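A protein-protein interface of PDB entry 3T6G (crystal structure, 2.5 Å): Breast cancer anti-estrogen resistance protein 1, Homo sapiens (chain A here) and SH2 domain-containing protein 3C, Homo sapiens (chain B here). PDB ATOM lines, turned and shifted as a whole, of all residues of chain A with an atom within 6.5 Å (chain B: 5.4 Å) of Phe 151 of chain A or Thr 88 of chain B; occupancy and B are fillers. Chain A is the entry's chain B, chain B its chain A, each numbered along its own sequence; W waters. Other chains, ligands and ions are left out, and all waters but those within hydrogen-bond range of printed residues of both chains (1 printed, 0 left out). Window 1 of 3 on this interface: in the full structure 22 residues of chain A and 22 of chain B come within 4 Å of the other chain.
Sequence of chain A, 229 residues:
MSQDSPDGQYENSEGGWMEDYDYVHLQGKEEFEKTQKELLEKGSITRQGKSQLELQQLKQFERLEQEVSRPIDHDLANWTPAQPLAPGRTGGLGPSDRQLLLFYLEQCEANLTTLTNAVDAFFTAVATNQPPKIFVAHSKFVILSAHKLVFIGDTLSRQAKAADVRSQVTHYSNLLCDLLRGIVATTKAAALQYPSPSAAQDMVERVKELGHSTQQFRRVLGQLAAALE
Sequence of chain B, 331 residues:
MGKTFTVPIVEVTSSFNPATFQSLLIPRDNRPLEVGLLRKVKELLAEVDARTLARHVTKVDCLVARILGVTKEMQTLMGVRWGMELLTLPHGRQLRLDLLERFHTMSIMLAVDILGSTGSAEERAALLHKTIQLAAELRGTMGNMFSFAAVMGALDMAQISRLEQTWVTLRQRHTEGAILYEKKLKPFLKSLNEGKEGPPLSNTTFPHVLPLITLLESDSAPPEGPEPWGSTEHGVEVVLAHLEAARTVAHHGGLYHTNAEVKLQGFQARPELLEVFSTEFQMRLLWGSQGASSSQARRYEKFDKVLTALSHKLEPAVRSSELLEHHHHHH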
ATOM      1  N   ALA A 146      13.168   1.143  37.774  1.00  0.00           N
ATOM      2  CA  ALA A 146      14.272   0.207  37.826  1.00  0.00           C
ATOM      3  C   ALA A 146      14.724  -0.110  36.430  1.00  0.00           C
ATOM      4  O   ALA A 146      15.898  -0.409  36.233  1.00  0.00           O
ATOM      5  CB  ALA A 146      13.876  -1.090  38.560  1.00  0.00           C
ATOM      6  N   HIS A 147      13.795  -0.068  35.469  1.00  0.00           N
ATOM      7  CA  HIS A 147      14.166  -0.316  34.072  1.00  0.00           C
ATOM      8  C   HIS A 147      15.104   0.765  33.516  1.00  0.00           C
ATOM      9  O   HIS A 147      15.917   0.491  32.645  1.00  0.00           O
ATOM     10  CB  HIS A 147      12.966  -0.541  33.149  1.00  0.00           C
ATOM     11  CG  HIS A 147      13.272  -1.487  32.031  1.00  0.00           C
ATOM     12  ND1 HIS A 147      14.006  -1.117  30.922  1.00  0.00           N
ATOM     13  CD2 HIS A 147      13.001  -2.804  31.880  1.00  0.00           C
ATOM     14  CE1 HIS A 147      14.163  -2.165  30.133  1.00  0.00           C
ATOM     15  NE2 HIS A 147      13.566  -3.203  30.690  1.00  0.00           N
ATOM     16  N   LYS A 148      15.006   1.978  34.045  1.00  0.00           N
ATOM     17  CA  LYS A 148      15.961   3.023  33.708  1.00  0.00           C
ATOM     18  C   LYS A 148      17.382   2.512  33.879  1.00  0.00           C
ATOM     19  O   LYS A 148      18.261   2.909  33.134  1.00  0.00           O
ATOM     20  CB  LYS A 148      15.742   4.275  34.562  1.00  0.00           C
ATOM     21  CG  LYS A 148      14.349   4.858  34.361  1.00  0.00           C
ATOM     22  CD  LYS A 148      14.135   6.223  35.016  1.00  0.00           C
ATOM     23  CE  LYS A 148      12.751   6.773  34.613  1.00  0.00           C
ATOM     24  NZ  LYS A 148      12.272   7.882  35.486  1.00  0.00           N
ATOM     25  N   LEU A 149      17.600   1.618  34.838  1.00  0.00           N
ATOM     26  CA  LEU A 149      18.942   1.115  35.114  1.00  0.00           C
ATOM     27  C   LEU A 149      19.320   0.081  34.093  1.00  0.00           C
ATOM     28  O   LEU A 149      20.491  -0.026  33.713  1.00  0.00           O
ATOM     29  CB  LEU A 149      19.036   0.464  36.502  1.00  0.00           C
ATOM     30  CG  LEU A 149      19.676   1.256  37.624  1.00  0.00           C
ATOM     31  CD1 LEU A 149      19.053   2.635  37.706  1.00  0.00           C
ATOM     32  CD2 LEU A 149      19.509   0.494  38.952  1.00  0.00           C
ATOM     33  N   VAL A 150      18.345  -0.728  33.679  1.00  0.00           N
ATOM     34  CA  VAL A 150      18.653  -1.728  32.663  1.00  0.00           C
ATOM     35  C   VAL A 150      19.180  -1.047  31.377  1.00  0.00           C
ATOM     36  O   VAL A 150      20.073  -1.576  30.716  1.00  0.00           O
ATOM     37  CB  VAL A 150      17.456  -2.588  32.316  1.00  0.00           C
ATOM     38  CG1 VAL A 150      17.794  -3.457  31.113  1.00  0.00           C
ATOM     39  CG2 VAL A 150      17.088  -3.463  33.511  1.00  0.00           C
ATOM     40  N   PHE A 151      18.628   0.125  31.053  1.00  0.00           N
ATOM     41  CA  PHE A 151      18.953   0.848  29.836  1.00  0.00           C
ATOM     42  C   PHE A 151      20.369   1.396  29.938  1.00  0.00           C
ATOM     43  O   PHE A 151      21.185   1.250  29.025  1.00  0.00           O
ATOM     44  CB  PHE A 151      17.966   1.994  29.656  1.00  0.00           C
ATOM     45  CG  PHE A 151      16.625   1.563  29.136  1.00  0.00           C
ATOM     46  CD1 PHE A 151      16.530   0.529  28.213  1.00  0.00           C
ATOM     47  CD2 PHE A 151      15.464   2.213  29.545  1.00  0.00           C
ATOM     48  CE1 PHE A 151      15.294   0.136  27.686  1.00  0.00           C
ATOM     49  CE2 PHE A 151      14.224   1.843  29.029  1.00  0.00           C
ATOM     50  CZ  PHE A 151      14.140   0.790  28.096  1.00  0.00           C
ATOM     51  N   ILE A 152      20.644   2.019  31.075  1.00  0.00           N
ATOM     52  CA  ILE A 152      21.967   2.514  31.384  1.00  0.00           C
ATOM     53  C   ILE A 152      22.990   1.392  31.247  1.00  0.00           C
ATOM     54  O   ILE A 152      24.020   1.559  30.603  1.00  0.00           O
ATOM     55  CB  ILE A 152      22.011   3.088  32.800  1.00  0.00           C
ATOM     56  CG1 ILE A 152      21.571   4.553  32.778  1.00  0.00           C
ATOM     57  CG2 ILE A 152      23.393   2.955  33.359  1.00  0.00           C
ATOM     58  CD1 ILE A 152      20.792   4.989  33.999  1.00  0.00           C
ATOM     59  N   GLY A 153      22.693   0.238  31.830  1.00  0.00           N
ATOM     60  CA  GLY A 153      23.601  -0.891  31.753  1.00  0.00           C
ATOM     61  C   GLY A 153      23.851  -1.357  30.335  1.00  0.00           C
ATOM     62  O   GLY A 153      24.945  -1.818  30.013  1.00  0.00           O
ATOM     63  N   ASP A 154      22.831  -1.233  29.491  1.00  0.00           N
ATOM     64  CA  ASP A 154      22.895  -1.653  28.098  1.00  0.00           C
ATOM     65  C   ASP A 154      23.804  -0.728  27.294  1.00  0.00           C
ATOM     66  O   ASP A 154      24.692  -1.183  26.580  1.00  0.00           O
ATOM     67  CB  ASP A 154      21.494  -1.671  27.499  1.00  0.00           C
ATOM     68  CG  ASP A 154      20.686  -2.915  27.906  1.00  0.00           C
ATOM     69  OD1 ASP A 154      21.271  -3.890  28.438  1.00  0.00           O
ATOM     70  OD2 ASP A 154      19.461  -2.909  27.679  1.00  0.00           O
ATOM     71  N   THR A 155      23.573   0.573  27.414  1.00  0.00           N
ATOM     72  CA  THR A 155      24.495   1.558  26.887  1.00  0.00           C
ATOM     73  C   THR A 155      25.937   1.250  27.307  1.00  0.00           C
ATOM     74  O   THR A 155      26.833   1.213  26.470  1.00  0.00           O
ATOM     75  CB  THR A 155      24.164   2.948  27.397  1.00  0.00           C
ATOM     76  OG1 THR A 155      23.049   3.448  26.676  1.00  0.00           O
ATOM     77  CG2 THR A 155      25.344   3.883  27.177  1.00  0.00           C
ATOM     78  N   LEU A 156      26.174   1.054  28.600  1.00  0.00           N
ATOM     79  CA  LEU A 156      27.529   0.741  29.037  1.00  0.00           C
ATOM     80  C   LEU A 156      28.014  -0.553  28.392  1.00  0.00           C
ATOM     81  O   LEU A 156      29.204  -0.708  28.121  1.00  0.00           O
ATOM     82  CB  LEU A 156      27.612   0.658  30.541  1.00  0.00           C
ATOM     83  CG  LEU A 156      27.438   1.989  31.255  1.00  0.00           C
ATOM     84  CD1 LEU A 156      27.069   1.726  32.697  1.00  0.00           C
ATOM     85  CD2 LEU A 156      28.729   2.793  31.160  1.00  0.00           C
ATOM     86  N   ARG A 158      27.453  -1.361  25.460  1.00  0.00           N
ATOM     87  CA  ARG A 158      27.757  -1.038  24.064  1.00  0.00           C
ATOM     88  C   ARG A 158      29.013  -0.174  23.881  1.00  0.00           C
ATOM     89  O   ARG A 158      29.899  -0.531  23.119  1.00  0.00           O
ATOM     90  CB  ARG A 158      26.543  -0.422  23.377  1.00  0.00           C
ATOM     91  CG  ARG A 158      25.510  -1.460  23.035  1.00  0.00           C
ATOM     92  CD  ARG A 158      24.345  -0.862  22.280  1.00  0.00           C
ATOM     93  NE  ARG A 158      23.457  -0.053  23.112  1.00  0.00           N
ATOM     94  CZ  ARG A 158      22.354  -0.520  23.687  1.00  0.00           C
ATOM     95  NH1 ARG A 158      22.025  -1.795  23.530  1.00  0.00           N
ATOM     96  NH2 ARG A 158      21.583   0.285  24.413  1.00  0.00           N
ATOM     97  N   SER A 173      22.541  -6.010  33.820  1.00  0.00           N
ATOM     98  CA  SER A 173      21.361  -5.598  33.060  1.00  0.00           C
ATOM     99  C   SER A 173      20.443  -6.779  32.790  1.00  0.00           C
ATOM    100  O   SER A 173      19.247  -6.691  33.001  1.00  0.00           O
ATOM    101  CB  SER A 173      21.760  -4.965  31.742  1.00  0.00           C
ATOM    102  OG  SER A 173      22.108  -3.606  31.942  1.00  0.00           O
ATOM    103  N   MET B  84      18.029   6.578  18.816  1.00  0.00           N
ATOM    104  CA  MET B  84      17.152   5.537  19.295  1.00  0.00           C
ATOM    105  C   MET B  84      17.629   5.087  20.649  1.00  0.00           C
ATOM    106  O   MET B  84      16.816   4.843  21.548  1.00  0.00           O
ATOM    107  CB  MET B  84      17.096   4.351  18.326  1.00  0.00           C
ATOM    108  CG  MET B  84      16.266   4.587  17.045  1.00  0.00           C
ATOM    109  SD  MET B  84      14.555   5.136  17.315  1.00  0.00           S
ATOM    110  CE  MET B  84      14.755   6.903  17.293  1.00  0.00           C
ATOM    111  N   GLU B  85      18.948   4.963  20.785  1.00  0.00           N
ATOM    112  CA  GLU B  85      19.568   4.594  22.054  1.00  0.00           C
ATOM    113  C   GLU B  85      19.421   5.735  23.038  1.00  0.00           C
ATOM    114  O   GLU B  85      19.040   5.533  24.190  1.00  0.00           O
ATOM    115  CB  GLU B  85      21.034   4.247  21.859  1.00  0.00           C
ATOM    116  CG  GLU B  85      21.775   3.982  23.143  1.00  0.00           C
ATOM    117  CD  GLU B  85      22.969   3.064  22.925  1.00  0.00           C
ATOM    118  OE1 GLU B  85      23.239   2.744  21.745  1.00  0.00           O
ATOM    119  OE2 GLU B  85      23.624   2.661  23.920  1.00  0.00           O
ATOM    120  N   LEU B  86      19.659   6.947  22.561  1.00  0.00           N
ATOM    121  CA  LEU B  86      19.604   8.114  23.433  1.00  0.00           C
ATOM    122  C   LEU B  86      18.270   8.256  24.154  1.00  0.00           C
ATOM    123  O   LEU B  86      18.230   8.704  25.296  1.00  0.00           O
ATOM    124  CB  LEU B  86      19.933   9.410  22.675  1.00  0.00           C
ATOM    125  CG  LEU B  86      19.898  10.625  23.616  1.00  0.00           C
ATOM    126  CD1 LEU B  86      20.954  10.455  24.712  1.00  0.00           C
ATOM    127  CD2 LEU B  86      20.091  11.967  22.920  1.00  0.00           C
ATOM    128  N   LEU B  87      17.171   7.891  23.501  1.00  0.00           N
ATOM    129  CA  LEU B  87      15.857   8.153  24.104  1.00  0.00           C
ATOM    130  C   LEU B  87      15.390   7.145  25.170  1.00  0.00           C
ATOM    131  O   LEU B  87      14.317   7.312  25.745  1.00  0.00           O
ATOM    132  CB  LEU B  87      14.779   8.428  23.043  1.00  0.00           C
ATOM    133  CG  LEU B  87      14.671   7.498  21.842  1.00  0.00           C
ATOM    134  CD1 LEU B  87      14.087   6.185  22.269  1.00  0.00           C
ATOM    135  CD2 LEU B  87      13.800   8.138  20.793  1.00  0.00           C
ATOM    136  N   THR B  88      16.201   6.122  25.435  1.00  0.00           N
ATOM    137  CA  THR B  88      15.971   5.240  26.572  1.00  0.00           C
ATOM    138  C   THR B  88      16.711   5.738  27.816  1.00  0.00           C
ATOM    139  O   THR B  88      16.373   5.373  28.937  1.00  0.00           O
ATOM    140  CB  THR B  88      16.478   3.821  26.295  1.00  0.00           C
ATOM    141  OG1 THR B  88      17.906   3.799  26.404  1.00  0.00           O
ATOM    142  CG2 THR B  88      16.053   3.347  24.912  1.00  0.00           C
ATOM    143  N   LEU B  89      17.734   6.556  27.607  1.00  0.00           N
ATOM    144  CA  LEU B  89      18.607   7.015  28.680  1.00  0.00           C
ATOM    145  C   LEU B  89      18.048   8.237  29.403  1.00  0.00           C
ATOM    146  O   LEU B  89      17.243   8.972  28.857  1.00  0.00           O
ATOM    147  CB  LEU B  89      20.008   7.312  28.141  1.00  0.00           C
ATOM    148  CG  LEU B  89      20.869   6.079  27.914  1.00  0.00           C
ATOM    149  CD1 LEU B  89      20.203   4.900  28.557  1.00  0.00           C
ATOM    150  CD2 LEU B  89      21.067   5.828  26.443  1.00  0.00           C
ATOM    151  N   PRO B  90      18.487   8.470  30.647  1.00  0.00           N
ATOM    152  CA  PRO B  90      17.727   9.450  31.417  1.00  0.00           C
ATOM    153  C   PRO B  90      17.989  10.835  30.862  1.00  0.00           C
ATOM    154  O   PRO B  90      17.158  11.726  31.026  1.00  0.00           O
ATOM    155  CB  PRO B  90      18.308   9.318  32.832  1.00  0.00           C
ATOM    156  CG  PRO B  90      19.328   8.208  32.754  1.00  0.00           C
ATOM    157  CD  PRO B  90      19.736   8.106  31.325  1.00  0.00           C
ATOM    158  N   ARG B  96      13.335  13.054  23.801  1.00  0.00           N
ATOM    159  CA  ARG B  96      11.978  12.552  24.024  1.00  0.00           C
ATOM    160  C   ARG B  96      10.926  13.670  24.001  1.00  0.00           C
ATOM    161  O   ARG B  96       9.839  13.517  23.427  1.00  0.00           O
ATOM    162  CB  ARG B  96      11.882  11.815  25.352  1.00  0.00           C
ATOM    163  CG  ARG B  96      12.320  10.369  25.318  1.00  0.00           C
ATOM    164  CD  ARG B  96      12.000   9.699  26.667  1.00  0.00           C
ATOM    165  NE  ARG B  96      12.705  10.357  27.765  1.00  0.00           N
ATOM    166  CZ  ARG B  96      13.846   9.911  28.276  1.00  0.00           C
ATOM    167  NH1 ARG B  96      14.394   8.806  27.794  1.00  0.00           N
ATOM    168  NH2 ARG B  96      14.443  10.572  29.252  1.00  0.00           N
ATOM    169  N   LEU B 212       6.862   3.994  24.620  1.00  0.00           N
ATOM    170  CA  LEU B 212       8.053   4.216  25.448  1.00  0.00           C
ATOM    171  C   LEU B 212       8.276   5.675  25.896  1.00  0.00           C
ATOM    172  O   LEU B 212       8.357   5.961  27.081  1.00  0.00           O
ATOM    173  CB  LEU B 212       9.295   3.750  24.710  1.00  0.00           C
ATOM    174  CG  LEU B 212      10.614   4.147  25.380  1.00  0.00           C
ATOM    175  CD1 LEU B 212      10.793   3.382  26.710  1.00  0.00           C
ATOM    176  CD2 LEU B 212      11.788   3.879  24.453  1.00  0.00           C
ATOM    177  N   LEU B 216       8.283   6.993  29.922  1.00  0.00           N
ATOM    178  CA  LEU B 216       9.418   7.611  30.601  1.00  0.00           C
ATOM    179  C   LEU B 216       9.218   9.083  30.926  1.00  0.00           C
ATOM    180  O   LEU B 216      10.025   9.674  31.635  1.00  0.00           O
ATOM    181  CB  LEU B 216      10.702   7.463  29.801  1.00  0.00           C
ATOM    182  CG  LEU B 216      11.000   6.170  29.040  1.00  0.00           C
ATOM    183  CD1 LEU B 216      12.471   6.140  28.603  1.00  0.00           C
ATOM    184  CD2 LEU B 216      10.666   4.970  29.872  1.00  0.00           C
ATOM    185  N   LEU B 243       8.942  -1.744  27.463  1.00  0.00           N
ATOM    186  CA  LEU B 243      10.295  -1.537  27.978  1.00  0.00           C
ATOM    187  C   LEU B 243      11.271  -2.588  27.465  1.00  0.00           C
ATOM    188  O   LEU B 243      12.381  -2.270  27.063  1.00  0.00           O
ATOM    189  CB  LEU B 243      10.317  -1.510  29.499  1.00  0.00           C
ATOM    190  CG  LEU B 243       9.648  -0.321  30.173  1.00  0.00           C
ATOM    191  CD1 LEU B 243       9.494  -0.614  31.681  1.00  0.00           C
ATOM    192  CD2 LEU B 243      10.436   0.956  29.942  1.00  0.00           C
ATOM    193  N   ALA B 246      12.033  -1.960  23.939  1.00  0.00           N
ATOM    194  CA  ALA B 246      12.808  -0.776  23.687  1.00  0.00           C
ATOM    195  C   ALA B 246      14.281  -1.134  23.693  1.00  0.00           C
ATOM    196  O   ALA B 246      15.108  -0.373  23.216  1.00  0.00           O
ATOM    197  CB  ALA B 246      12.491   0.290  24.698  1.00  0.00           C
ATOM    198  N   ARG B 247      14.617  -2.306  24.213  1.00  0.00           N
ATOM    199  CA  ARG B 247      16.022  -2.683  24.263  1.00  0.00           C
ATOM    200  C   ARG B 247      16.432  -3.206  22.900  1.00  0.00           C
ATOM    201  O   ARG B 247      17.577  -3.048  22.492  1.00  0.00           O
ATOM    202  CB  ARG B 247      16.294  -3.758  25.318  1.00  0.00           C
ATOM    203  CG  ARG B 247      15.908  -3.392  26.723  1.00  0.00           C
ATOM    204  CD  ARG B 247      16.005  -4.632  27.608  1.00  0.00           C
ATOM    205  NE  ARG B 247      17.343  -4.802  28.148  1.00  0.00           N
ATOM    206  CZ  ARG B 247      17.907  -5.977  28.430  1.00  0.00           C
ATOM    207  NH1 ARG B 247      17.253  -7.103  28.178  1.00  0.00           N
ATOM    208  NH2 ARG B 247      19.140  -6.026  28.954  1.00  0.00           N
ATOM    209  N   ALA B 250      17.004   0.025  20.858  1.00  0.00           N
ATOM    210  CA  ALA B 250      18.224   0.755  21.146  1.00  0.00           C
ATOM    211  C   ALA B 250      19.412  -0.012  20.579  1.00  0.00           C
ATOM    212  O   ALA B 250      20.395   0.570  20.116  1.00  0.00           O
ATOM    213  CB  ALA B 250      18.378   0.989  22.657  1.00  0.00           C
HETATM  214  O   HOH W   1      19.740   1.734  26.255  1.00  0.00           O
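The guanidinium group (NE) of Arg 247 of chain B lies within salt-bridge range of the side-chain carboxylate (OD2) of Asp 154 of chain A, at 2.9 Å. The side-chain carboxylate (OE2) of Glu 85 of chain B is in hydrogen-bond range of the side-chain hydroxyl (OG1) of Thr 155 of chain A (2.9 Å). The guanidinium group of Arg 158 of chain A is in salt-bridge range of the side-chain carboxylate of Glu 85 of chain B, 2.8 Å away.
The side-chain hydroxyl (OG) of Ser 173 of chain A is in hydrogen-bond range of the backbone carbonyl oxygen (O) of Val 150 of chain A, at 3.1 Å. The backbone NH of Asp 154 of chain A lies within hydrogen-bond range of the side-chain hydroxyl of Ser 173 of chain A, 3.5 Å away. The guanidinium group (NH2) of Arg 96 of chain B lies within hydrogen-bond range of the backbone carbonyl oxygen (O) of Pro 90 of chain B (3.4 Å). The backbone carbonyl oxygen of Leu 89 of chain B lies within hydrogen-bond range of the guanidinium group of Arg 96 of chain B, at 3.0 Å. The side-chain hydroxyl (OG1) of Thr 88 of chain B lies within hydrogen-bond range of the backbone carbonyl oxygen (O) of Glu 85 of chain B (3.0 Å).
CE1 of His 147 of chain A touches O of Leu 243 of chain B, at 3.6 Å. His 147 of chain A touches Arg 247 of chain B (CE1 to CD, 3.98 Å). CD1 of Leu 89 of chain B touches C of Phe 151 of chain A, 3.8 Å away. O of Leu 243 of chain B touches CZ of Phe 151 of chain A, at 3.7 Å. Ala 246 of chain B touches Phe 151 of chain A (CB to CZ, 3.8 Å). Ile 152 of chain A touches Leu 89 of chain B. CD1 of Ile 152 of chain A touches CG of Pro 90 of chain B (3.7 Å). Thr 155 of chain A touches Leu 89 of chain B (OG1 to CD2, 3.1 Å). CB of Ala 250 of chain B touches NH2 of Arg 158 of chain A, at 3.7 Å. Ser 173 of chain A touches Arg 247 of chain B (CB to NH2, 3.97 Å).
Of the printed residues of chain B, Phe 151 of chain A touches Thr 88, Leu 89, Leu 243, Ala 246 and Arg 247. Of the printed residues of chain B, Ile 152 of chain A touches Leu 89 (3.9 Å) and Pro 90 (3.7 Å). Printed residues of chain B within 4 Å of Thr 155 of chain A: Glu 85 (2.9 Å) and Leu 89 (3.1 Å). Leu 156 of chain A touches none of the printed residues of chain B. Printed residues of chain B within 4 Å of Arg 158 of chain A: Glu 85 and Ala 250. Leu 87 of chain B touches none of the printed residues of chain A. Of chain A, only Phe 151 (3.3 Å) comes within 4 Å of Thr 88 of chain B. The nearest printed residue of chain B that does not touch Thr 155 of chain A is Thr 88 of chain B (5.2 Å).
Printed residues of chain A that touch a printed residue of chain B: His 147, Val 150, Phe 151, Ile 152, Asp 154, Thr 155, Arg 158 and Ser 173. Hydrophobic or aromatic side chains of chain A within 4 Å of the printed part of chain B: His 147, Val 150, Phe 151 and Ile 152. Along chain B the printed residues that touch a printed residue of chain A span positions 85 to 250. Among the printed residues, Asp or Glu carboxylates within 4 Å of a Lys or Arg side-chain nitrogen of the other chain: Asp 154 of chain A with Arg 247 of chain B (2.9 Å) and Arg 158 of chain A with Glu 85 of chain B (2.8 Å).
Water W1 lies within hydrogen-bond range of OG1 of Thr 88 of chain B (2.8 Å), NH2 of Arg 158 of chain A (3.0 Å) and O of Phe 151 of chain A (3.2 Å).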
